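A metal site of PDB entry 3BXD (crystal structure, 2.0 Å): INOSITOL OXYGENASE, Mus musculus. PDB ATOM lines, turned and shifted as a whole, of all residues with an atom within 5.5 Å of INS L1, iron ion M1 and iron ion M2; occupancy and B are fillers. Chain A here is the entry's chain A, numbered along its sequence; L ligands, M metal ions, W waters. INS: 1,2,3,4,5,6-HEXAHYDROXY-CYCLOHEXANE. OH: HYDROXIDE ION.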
ATOM      1  N   ARG A  33     -23.687 -22.472   6.452  1.00  0.00           N
ATOM      2  CA  ARG A  33     -22.253 -22.681   6.497  1.00  0.00           C
ATOM      3  C   ARG A  33     -21.958 -24.147   6.770  1.00  0.00           C
ATOM      4  O   ARG A  33     -21.104 -24.485   7.589  1.00  0.00           O
ATOM      5  CB  ARG A  33     -21.663 -21.773   7.573  1.00  0.00           C
ATOM      6  CG  ARG A  33     -20.214 -21.972   7.887  1.00  0.00           C
ATOM      7  CD  ARG A  33     -19.575 -20.652   8.282  1.00  0.00           C
ATOM      8  NE  ARG A  33     -19.174 -19.901   7.106  1.00  0.00           N
ATOM      9  CZ  ARG A  33     -17.959 -19.936   6.570  1.00  0.00           C
ATOM     10  NH1 ARG A  33     -16.998 -20.669   7.128  1.00  0.00           N
ATOM     11  NH2 ARG A  33     -17.691 -19.227   5.489  1.00  0.00           N
ATOM     12  N   TYR A  35     -20.440 -27.571   5.744  1.00  0.00           N
ATOM     13  CA  TYR A  35     -19.413 -28.128   4.879  1.00  0.00           C
ATOM     14  C   TYR A  35     -19.312 -29.639   5.016  1.00  0.00           C
ATOM     15  O   TYR A  35     -18.367 -30.274   4.519  1.00  0.00           O
ATOM     16  CB  TYR A  35     -18.057 -27.483   5.183  1.00  0.00           C
ATOM     17  CG  TYR A  35     -18.045 -25.991   4.944  1.00  0.00           C
ATOM     18  CD1 TYR A  35     -18.133 -25.486   3.654  1.00  0.00           C
ATOM     19  CD2 TYR A  35     -17.954 -25.098   6.001  1.00  0.00           C
ATOM     20  CE1 TYR A  35     -18.124 -24.117   3.425  1.00  0.00           C
ATOM     21  CE2 TYR A  35     -17.942 -23.734   5.780  1.00  0.00           C
ATOM     22  CZ  TYR A  35     -18.032 -23.256   4.498  1.00  0.00           C
ATOM     23  OH  TYR A  35     -18.020 -21.892   4.276  1.00  0.00           O
ATOM     24  N   TYR A  48     -12.186 -24.708  -2.948  1.00  0.00           N
ATOM     25  CA  TYR A  48     -11.306 -24.383  -1.813  1.00  0.00           C
ATOM     26  C   TYR A  48     -10.038 -25.218  -1.881  1.00  0.00           C
ATOM     27  O   TYR A  48      -8.975 -24.821  -1.395  1.00  0.00           O
ATOM     28  CB  TYR A  48     -11.996 -24.659  -0.474  1.00  0.00           C
ATOM     29  CG  TYR A  48     -12.772 -23.489   0.063  1.00  0.00           C
ATOM     30  CD1 TYR A  48     -12.119 -22.329   0.472  1.00  0.00           C
ATOM     31  CD2 TYR A  48     -14.147 -23.548   0.171  1.00  0.00           C
ATOM     32  CE1 TYR A  48     -12.832 -21.254   0.956  1.00  0.00           C
ATOM     33  CE2 TYR A  48     -14.870 -22.484   0.664  1.00  0.00           C
ATOM     34  CZ  TYR A  48     -14.197 -21.339   1.054  1.00  0.00           C
ATOM     35  OH  TYR A  48     -14.916 -20.286   1.539  1.00  0.00           O
ATOM     36  N   ASP A  89     -21.374 -16.679  -6.674  1.00  0.00           N
ATOM     37  CA  ASP A  89     -20.198 -17.076  -5.896  1.00  0.00           C
ATOM     38  C   ASP A  89     -20.148 -18.605  -5.735  1.00  0.00           C
ATOM     39  O   ASP A  89     -21.101 -19.222  -5.251  1.00  0.00           O
ATOM     40  CB  ASP A  89     -20.224 -16.355  -4.544  1.00  0.00           C
ATOM     41  CG  ASP A  89     -18.955 -16.563  -3.758  1.00  0.00           C
ATOM     42  OD1 ASP A  89     -18.355 -17.648  -3.877  1.00  0.00           O
ATOM     43  OD2 ASP A  89     -18.564 -15.639  -3.007  1.00  0.00           O
ATOM     44  N   SER A  91     -17.994 -20.476  -3.993  1.00  0.00           N
ATOM     45  CA  SER A  91     -17.554 -20.958  -2.690  1.00  0.00           C
ATOM     46  C   SER A  91     -18.661 -20.947  -1.640  1.00  0.00           C
ATOM     47  O   SER A  91     -18.525 -21.568  -0.590  1.00  0.00           O
ATOM     48  CB  SER A  91     -16.398 -20.099  -2.179  1.00  0.00           C
ATOM     49  OG  SER A  91     -16.839 -18.782  -1.924  1.00  0.00           O
ATOM     50  N   ASP A  92     -19.749 -20.232  -1.911  1.00  0.00           N
ATOM     51  CA  ASP A  92     -20.823 -20.047  -0.940  1.00  0.00           C
ATOM     52  C   ASP A  92     -21.826 -21.206  -1.000  1.00  0.00           C
ATOM     53  O   ASP A  92     -22.472 -21.415  -2.021  1.00  0.00           O
ATOM     54  CB  ASP A  92     -21.539 -18.720  -1.209  1.00  0.00           C
ATOM     55  CG  ASP A  92     -22.187 -18.130   0.036  1.00  0.00           C
ATOM     56  OD1 ASP A  92     -22.300 -18.828   1.068  1.00  0.00           O
ATOM     57  OD2 ASP A  92     -22.589 -16.943  -0.017  1.00  0.00           O
ATOM     58  N   PRO A  93     -21.959 -21.956   0.121  1.00  0.00           N
ATOM     59  CA  PRO A  93     -22.888 -23.087   0.187  1.00  0.00           C
ATOM     60  C   PRO A  93     -24.334 -22.658   0.435  1.00  0.00           C
ATOM     61  O   PRO A  93     -25.215 -23.511   0.499  1.00  0.00           O
ATOM     62  CB  PRO A  93     -22.381 -23.902   1.392  1.00  0.00           C
ATOM     63  CG  PRO A  93     -21.124 -23.199   1.881  1.00  0.00           C
ATOM     64  CD  PRO A  93     -21.179 -21.805   1.363  1.00  0.00           C
ATOM     65  N   HIS A 102     -27.272 -10.174  -2.839  1.00  0.00           N
ATOM     66  CA  HIS A 102     -26.699 -10.416  -1.524  1.00  0.00           C
ATOM     67  C   HIS A 102     -26.161  -9.123  -0.911  1.00  0.00           C
ATOM     68  O   HIS A 102     -26.257  -8.925   0.302  1.00  0.00           O
ATOM     69  CB  HIS A 102     -25.574 -11.450  -1.599  1.00  0.00           C
ATOM     70  CG  HIS A 102     -24.602 -11.369  -0.463  1.00  0.00           C
ATOM     71  ND1 HIS A 102     -24.848 -11.950   0.771  1.00  0.00           N
ATOM     72  CD2 HIS A 102     -23.388 -10.779  -0.363  1.00  0.00           C
ATOM     73  CE1 HIS A 102     -23.835 -11.710   1.572  1.00  0.00           C
ATOM     74  NE2 HIS A 102     -22.931 -11.003   0.913  1.00  0.00           N
ATOM     75  N   THR A 106     -27.544  -7.711   2.735  1.00  0.00           N
ATOM     76  CA  THR A 106     -26.629  -7.515   3.845  1.00  0.00           C
ATOM     77  C   THR A 106     -26.763  -6.090   4.370  1.00  0.00           C
ATOM     78  O   THR A 106     -26.845  -5.859   5.573  1.00  0.00           O
ATOM     79  CB  THR A 106     -25.159  -7.785   3.449  1.00  0.00           C
ATOM     80  OG1 THR A 106     -25.011  -9.159   3.042  1.00  0.00           O
ATOM     81  CG2 THR A 106     -24.226  -7.513   4.614  1.00  0.00           C
ATOM     82  N   HIS A 127     -19.243  -4.519   0.703  1.00  0.00           N
ATOM     83  CA  HIS A 127     -18.205  -5.448   1.198  1.00  0.00           C
ATOM     84  C   HIS A 127     -17.725  -6.487   0.189  1.00  0.00           C
ATOM     85  O   HIS A 127     -16.562  -6.918   0.244  1.00  0.00           O
ATOM     86  CB  HIS A 127     -18.684  -6.139   2.474  1.00  0.00           C
ATOM     87  CG  HIS A 127     -19.653  -7.252   2.237  1.00  0.00           C
ATOM     88  ND1 HIS A 127     -21.005  -7.031   2.086  1.00  0.00           N
ATOM     89  CD2 HIS A 127     -19.470  -8.588   2.121  1.00  0.00           C
ATOM     90  CE1 HIS A 127     -21.613  -8.182   1.881  1.00  0.00           C
ATOM     91  NE2 HIS A 127     -20.692  -9.144   1.894  1.00  0.00           N
ATOM     92  N   ASP A 128     -18.590  -6.887  -0.734  1.00  0.00           N
ATOM     93  CA  ASP A 128     -18.239  -7.925  -1.699  1.00  0.00           C
ATOM     94  C   ASP A 128     -17.989  -7.421  -3.126  1.00  0.00           C
ATOM     95  O   ASP A 128     -17.981  -8.224  -4.064  1.00  0.00           O
ATOM     96  CB  ASP A 128     -19.343  -8.984  -1.750  1.00  0.00           C
ATOM     97  CG  ASP A 128     -19.172 -10.043  -0.688  1.00  0.00           C
ATOM     98  OD1 ASP A 128     -18.091 -10.079  -0.064  1.00  0.00           O
ATOM     99  OD2 ASP A 128     -20.111 -10.835  -0.494  1.00  0.00           O
ATOM    100  N   LYS A 131     -15.358  -8.790  -5.836  1.00  0.00           N
ATOM    101  CA  LYS A 131     -15.591  -9.986  -6.660  1.00  0.00           C
ATOM    102  C   LYS A 131     -15.779  -9.652  -8.135  1.00  0.00           C
ATOM    103  O   LYS A 131     -15.987 -10.549  -8.950  1.00  0.00           O
ATOM    104  CB  LYS A 131     -16.827 -10.736  -6.165  1.00  0.00           C
ATOM    105  CG  LYS A 131     -16.681 -11.303  -4.775  1.00  0.00           C
ATOM    106  CD  LYS A 131     -17.998 -11.805  -4.245  1.00  0.00           C
ATOM    107  CE  LYS A 131     -17.852 -12.353  -2.843  1.00  0.00           C
ATOM    108  NZ  LYS A 131     -19.168 -12.791  -2.322  1.00  0.00           N
ATOM    109  N   VAL A 144     -13.014 -15.237  -4.480  1.00  0.00           N
ATOM    110  CA  VAL A 144     -13.980 -15.473  -3.427  1.00  0.00           C
ATOM    111  C   VAL A 144     -13.473 -16.488  -2.407  1.00  0.00           C
ATOM    112  O   VAL A 144     -12.409 -17.086  -2.574  1.00  0.00           O
ATOM    113  CB  VAL A 144     -15.302 -16.016  -4.012  1.00  0.00           C
ATOM    114  CG1 VAL A 144     -15.849 -15.075  -5.063  1.00  0.00           C
ATOM    115  CG2 VAL A 144     -15.098 -17.405  -4.595  1.00  0.00           C
ATOM    116  N   GLY A 145     -14.257 -16.658  -1.341  1.00  0.00           N
ATOM    117  CA  GLY A 145     -14.016 -17.705  -0.365  1.00  0.00           C
ATOM    118  C   GLY A 145     -13.378 -17.227   0.915  1.00  0.00           C
ATOM    119  O   GLY A 145     -12.926 -16.086   1.029  1.00  0.00           O
ATOM    120  N   ASP A 146     -13.350 -18.118   1.909  1.00  0.00           N
ATOM    121  CA  ASP A 146     -12.650 -17.864   3.153  1.00  0.00           C
ATOM    122  C   ASP A 146     -11.179 -17.623   2.868  1.00  0.00           C
ATOM    123  O   ASP A 146     -10.599 -18.226   1.964  1.00  0.00           O
ATOM    124  CB  ASP A 146     -12.765 -19.068   4.091  1.00  0.00           C
ATOM    125  CG  ASP A 146     -14.158 -19.251   4.651  1.00  0.00           C
ATOM    126  OD1 ASP A 146     -15.020 -18.386   4.368  1.00  0.00           O
ATOM    127  OD2 ASP A 146     -14.386 -20.240   5.373  1.00  0.00           O
ATOM    128  N   THR A 147     -10.579 -16.745   3.663  1.00  0.00           N
ATOM    129  CA  THR A 147      -9.190 -16.410   3.515  1.00  0.00           C
ATOM    130  C   THR A 147      -8.369 -17.024   4.651  1.00  0.00           C
ATOM    131  O   THR A 147      -8.903 -17.433   5.678  1.00  0.00           O
ATOM    132  CB  THR A 147      -9.000 -14.902   3.554  1.00  0.00           C
ATOM    133  OG1 THR A 147      -9.703 -14.375   4.679  1.00  0.00           O
ATOM    134  CG2 THR A 147      -9.539 -14.275   2.263  1.00  0.00           C
ATOM    135  N   HIS A 198     -11.260 -10.816  -2.750  1.00  0.00           N
ATOM    136  CA  HIS A 198     -12.044  -9.588  -2.736  1.00  0.00           C
ATOM    137  C   HIS A 198     -11.826  -8.715  -1.505  1.00  0.00           C
ATOM    138  O   HIS A 198     -11.980  -7.495  -1.582  1.00  0.00           O
ATOM    139  CB  HIS A 198     -13.526  -9.924  -2.893  1.00  0.00           C
ATOM    140  CG  HIS A 198     -14.089 -10.747  -1.771  1.00  0.00           C
ATOM    141  ND1 HIS A 198     -13.664 -12.025  -1.506  1.00  0.00           N
ATOM    142  CD2 HIS A 198     -15.068 -10.482  -0.878  1.00  0.00           C
ATOM    143  CE1 HIS A 198     -14.345 -12.508  -0.489  1.00  0.00           C
ATOM    144  NE2 HIS A 198     -15.208 -11.588  -0.080  1.00  0.00           N
ATOM    145  N   ASP A 199     -11.448  -9.331  -0.379  1.00  0.00           N
ATOM    146  CA  ASP A 199     -11.243  -8.593   0.869  1.00  0.00           C
ATOM    147  C   ASP A 199     -10.160  -7.569   0.689  1.00  0.00           C
ATOM    148  O   ASP A 199     -10.393  -6.372   0.824  1.00  0.00           O
ATOM    149  CB  ASP A 199     -10.793  -9.507   2.007  1.00  0.00           C
ATOM    150  CG  ASP A 199     -11.905 -10.326   2.594  1.00  0.00           C
ATOM    151  OD1 ASP A 199     -12.854 -10.635   1.846  1.00  0.00           O
ATOM    152  OD2 ASP A 199     -11.824 -10.656   3.798  1.00  0.00           O
ATOM    153  N   HIS A 224     -13.252  -9.650   6.578  1.00  0.00           N
ATOM    154  CA  HIS A 224     -14.569 -10.255   6.783  1.00  0.00           C
ATOM    155  C   HIS A 224     -14.624 -11.714   6.319  1.00  0.00           C
ATOM    156  O   HIS A 224     -15.482 -12.477   6.766  1.00  0.00           O
ATOM    157  CB  HIS A 224     -15.666  -9.438   6.085  1.00  0.00           C
ATOM    158  CG  HIS A 224     -15.772  -9.695   4.613  1.00  0.00           C
ATOM    159  ND1 HIS A 224     -15.083  -8.958   3.673  1.00  0.00           N
ATOM    160  CD2 HIS A 224     -16.480 -10.616   3.914  1.00  0.00           C
ATOM    161  CE1 HIS A 224     -15.374  -9.400   2.468  1.00  0.00           C
ATOM    162  NE2 HIS A 224     -16.213 -10.423   2.592  1.00  0.00           N
ATOM    163  N   SER A 225     -13.706 -12.092   5.454  1.00  0.00           N
ATOM    164  CA  SER A 225     -13.635 -13.464   4.941  1.00  0.00           C
ATOM    165  C   SER A 225     -12.759 -14.369   5.807  1.00  0.00           C
ATOM    166  O   SER A 225     -12.685 -15.571   5.573  1.00  0.00           O
ATOM    167  CB  SER A 225     -13.079 -13.456   3.521  1.00  0.00           C
ATOM    168  OG  SER A 225     -13.832 -12.610   2.665  1.00  0.00           O
ATOM    169  N   PHE A 226     -12.103 -13.789   6.801  1.00  0.00           N
ATOM    170  CA  PHE A 226     -11.071 -14.487   7.556  1.00  0.00           C
ATOM    171  C   PHE A 226     -11.688 -15.324   8.694  1.00  0.00           C
ATOM    172  O   PHE A 226     -11.440 -15.079   9.876  1.00  0.00           O
ATOM    173  CB  PHE A 226     -10.054 -13.464   8.084  1.00  0.00           C
ATOM    174  CG  PHE A 226      -8.791 -14.075   8.629  1.00  0.00           C
ATOM    175  CD1 PHE A 226      -8.533 -15.426   8.483  1.00  0.00           C
ATOM    176  CD2 PHE A 226      -7.854 -13.287   9.266  1.00  0.00           C
ATOM    177  CE1 PHE A 226      -7.371 -15.985   8.979  1.00  0.00           C
ATOM    178  CE2 PHE A 226      -6.684 -13.843   9.773  1.00  0.00           C
ATOM    179  CZ  PHE A 226      -6.442 -15.181   9.617  1.00  0.00           C
ATOM    180  N   TYR A 227     -12.476 -16.325   8.309  1.00  0.00           N
ATOM    181  CA  TYR A 227     -13.272 -17.087   9.243  1.00  0.00           C
ATOM    182  C   TYR A 227     -12.429 -17.788  10.298  1.00  0.00           C
ATOM    183  O   TYR A 227     -12.757 -17.727  11.471  1.00  0.00           O
ATOM    184  CB  TYR A 227     -14.150 -18.110   8.512  1.00  0.00           C
ATOM    185  CG  TYR A 227     -15.514 -17.575   8.128  1.00  0.00           C
ATOM    186  CD1 TYR A 227     -15.681 -16.759   7.004  1.00  0.00           C
ATOM    187  CD2 TYR A 227     -16.636 -17.878   8.884  1.00  0.00           C
ATOM    188  CE1 TYR A 227     -16.931 -16.274   6.651  1.00  0.00           C
ATOM    189  CE2 TYR A 227     -17.894 -17.392   8.537  1.00  0.00           C
ATOM    190  CZ  TYR A 227     -18.034 -16.596   7.425  1.00  0.00           C
ATOM    191  OH  TYR A 227     -19.276 -16.114   7.067  1.00  0.00           O
ATOM    192  N   ASP A 257     -23.697 -10.652   7.384  1.00  0.00           N
ATOM    193  CA  ASP A 257     -23.115 -11.060   6.109  1.00  0.00           C
ATOM    194  C   ASP A 257     -23.654 -12.440   5.785  1.00  0.00           C
ATOM    195  O   ASP A 257     -24.091 -12.714   4.680  1.00  0.00           O
ATOM    196  CB  ASP A 257     -21.577 -11.072   6.215  1.00  0.00           C
ATOM    197  CG  ASP A 257     -20.893 -11.548   4.940  1.00  0.00           C
ATOM    198  OD1 ASP A 257     -21.522 -11.523   3.863  1.00  0.00           O
ATOM    199  OD2 ASP A 257     -19.704 -11.943   5.020  1.00  0.00           O
ATOM    200  N   LYS A 261     -28.589 -14.121   4.067  1.00  0.00           N
ATOM    201  CA  LYS A 261     -28.658 -14.851   2.801  1.00  0.00           C
ATOM    202  C   LYS A 261     -29.972 -15.634   2.681  1.00  0.00           C
ATOM    203  O   LYS A 261     -30.231 -16.540   3.472  1.00  0.00           O
ATOM    204  CB  LYS A 261     -27.442 -15.782   2.653  1.00  0.00           C
ATOM    205  CG  LYS A 261     -26.137 -15.043   2.350  1.00  0.00           C
ATOM    206  CD  LYS A 261     -24.913 -15.927   2.563  1.00  0.00           C
ATOM    207  CE  LYS A 261     -23.622 -15.144   2.374  1.00  0.00           C
ATOM    208  NZ  LYS A 261     -22.407 -15.919   2.740  1.00  0.00           N
HETATM  209  C1  INS L   1     -18.055 -14.330   1.079  1.00  0.00           C
HETATM  210  C2  INS L   1     -18.276 -15.638   0.302  1.00  0.00           C
HETATM  211  C3  INS L   1     -18.288 -16.820   1.261  1.00  0.00           C
HETATM  212  C4  INS L   1     -16.955 -16.880   1.989  1.00  0.00           C
HETATM  213  C5  INS L   1     -16.723 -15.593   2.772  1.00  0.00           C
HETATM  214  C6  INS L   1     -16.707 -14.397   1.834  1.00  0.00           C
HETATM  215  O1  INS L   1     -18.039 -13.244   0.170  1.00  0.00           O
HETATM  216  O2  INS L   1     -17.239 -15.814  -0.672  1.00  0.00           O
HETATM  217  O3  INS L   1     -18.460 -18.024   0.519  1.00  0.00           O
HETATM  218  O4  INS L   1     -17.013 -17.960   2.907  1.00  0.00           O
HETATM  219  O5  INS L   1     -15.478 -15.691   3.475  1.00  0.00           O
HETATM  220  O6  INS L   1     -16.482 -13.192   2.565  1.00  0.00           O
HETATM  221  O    OH L   2     -18.978 -12.011   2.743  1.00  0.00           O
HETATM  222 FE    FE M   1     -17.241 -11.643   1.181  1.00  0.00          FE
HETATM  223 FE    FE M   2     -20.709 -11.260   1.640  1.00  0.00          FE
HETATM  224  O   HOH W   1     -21.094 -13.374   0.911  1.00  0.00           O
HETATM  225  O   HOH W   2     -17.507 -20.499   1.353  1.00  0.00           O
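An oxygen (O4) of INS L1 is in hydrogen-bond range of the side-chain carboxylate (OD1) of Asp 146, at 2.5 Å. O2 of INS L1 sits at hydrogen-bond distance from OD2 of Asp 89, at 2.7 Å. O5 of INS L1 sits close to O of Ser 225. The side-chain hydroxyl of Ser 225 lies close to an oxygen (O6) of INS L1, 2.7 Å away. The side-chain amino group of Lys 131 sits close to an oxygen (O1) of INS L1 (2.8 Å). An oxygen (O4) of INS L1 is in hydrogen-bond range of the guanidinium group (NH2) of Arg 33. OG of Ser 91 lies within hydrogen-bond range of O3 of INS L1 (3.0 Å). N of Gly 145 lies within hydrogen-bond range of O2 of INS L1 (3.2 Å). An oxygen (O4) of INS L1 sits at hydrogen-bond distance from the side-chain hydroxyl of Tyr 48.
Water W2 lies within hydrogen-bond range of O of Ser 91, OH of Tyr 48, O3 of INS L1 and OH of Tyr 35.
Residues that only touch iron ion M1: Ser 225. Within 4 Å of iron ion M1: His 127, Asp 128, His 198, His 224 and Ser 225.
Four residues have an atom within 4 Å of iron ion M2: His 102, His 127, Asp 128 and Asp 257.
Iron ion M2 is bound by NE2 of His 127 (2.1 Å), O of OH L2 (2.2 Å), OD2 of Asp 128 (2.3 Å), water W1 (2.3 Å), NE2 of His 102 (2.4 Å) and OD1 of Asp 257 (2.4 Å). Iron ion M2 has six donor atoms within binding distance.
O1 of INS L1 binds iron ion M1. NE2 of His 224 binds iron ion M1 (2.1 Å). OD1 of Asp 128 binds iron ion M1 (2.2 Å). Iron ion M1 is bound by O6 of INS L1 (2.2 Å). O of OH L2 binds iron ion M1 (2.4 Å). NE2 of His 198 binds iron ion M1 (2.4 Å).
The backbone carbonyl oxygen of His 102 is in hydrogen-bond range of the side-chain hydroxyl of Thr 106 (3.0 Å). A ring nitrogen (NE2) of His 198 lies close to the side-chain carboxylate (OD1) of Asp 199. The backbone NH (N) of Asp 146 is in hydrogen-bond range of the side-chain hydroxyl (OH) of Tyr 48 (2.7 Å). The side-chain carboxylate (OD2) of Asp 89 is in salt-bridge range of the side-chain amino group (NZ) of Lys 131, 3.0 Å away. The backbone NH (N) of Ser 225 is in hydrogen-bond range of the side-chain carboxylate (OD2) of Asp 199 (2.9 Å). N of Thr 147 lies within hydrogen-bond range of O of Ser 225 (3.1 Å). OG of Ser 91 lies within hydrogen-bond range of N of Gly 145, at 3.4 Å. OD2 of Asp 92 lies within salt-bridge range of NZ of Lys 261, at 2.9 Å.
Residues that only touch INS L1: Asp 92 (3.4 Å), Val 144 (3.9 Å) and Tyr 227 (3.5 Å). Of the 24 residues printed, 14 come within 4 Å of INS L1. Along chain A the residues within 4 Å of INS L1 span positions 33 to 227.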
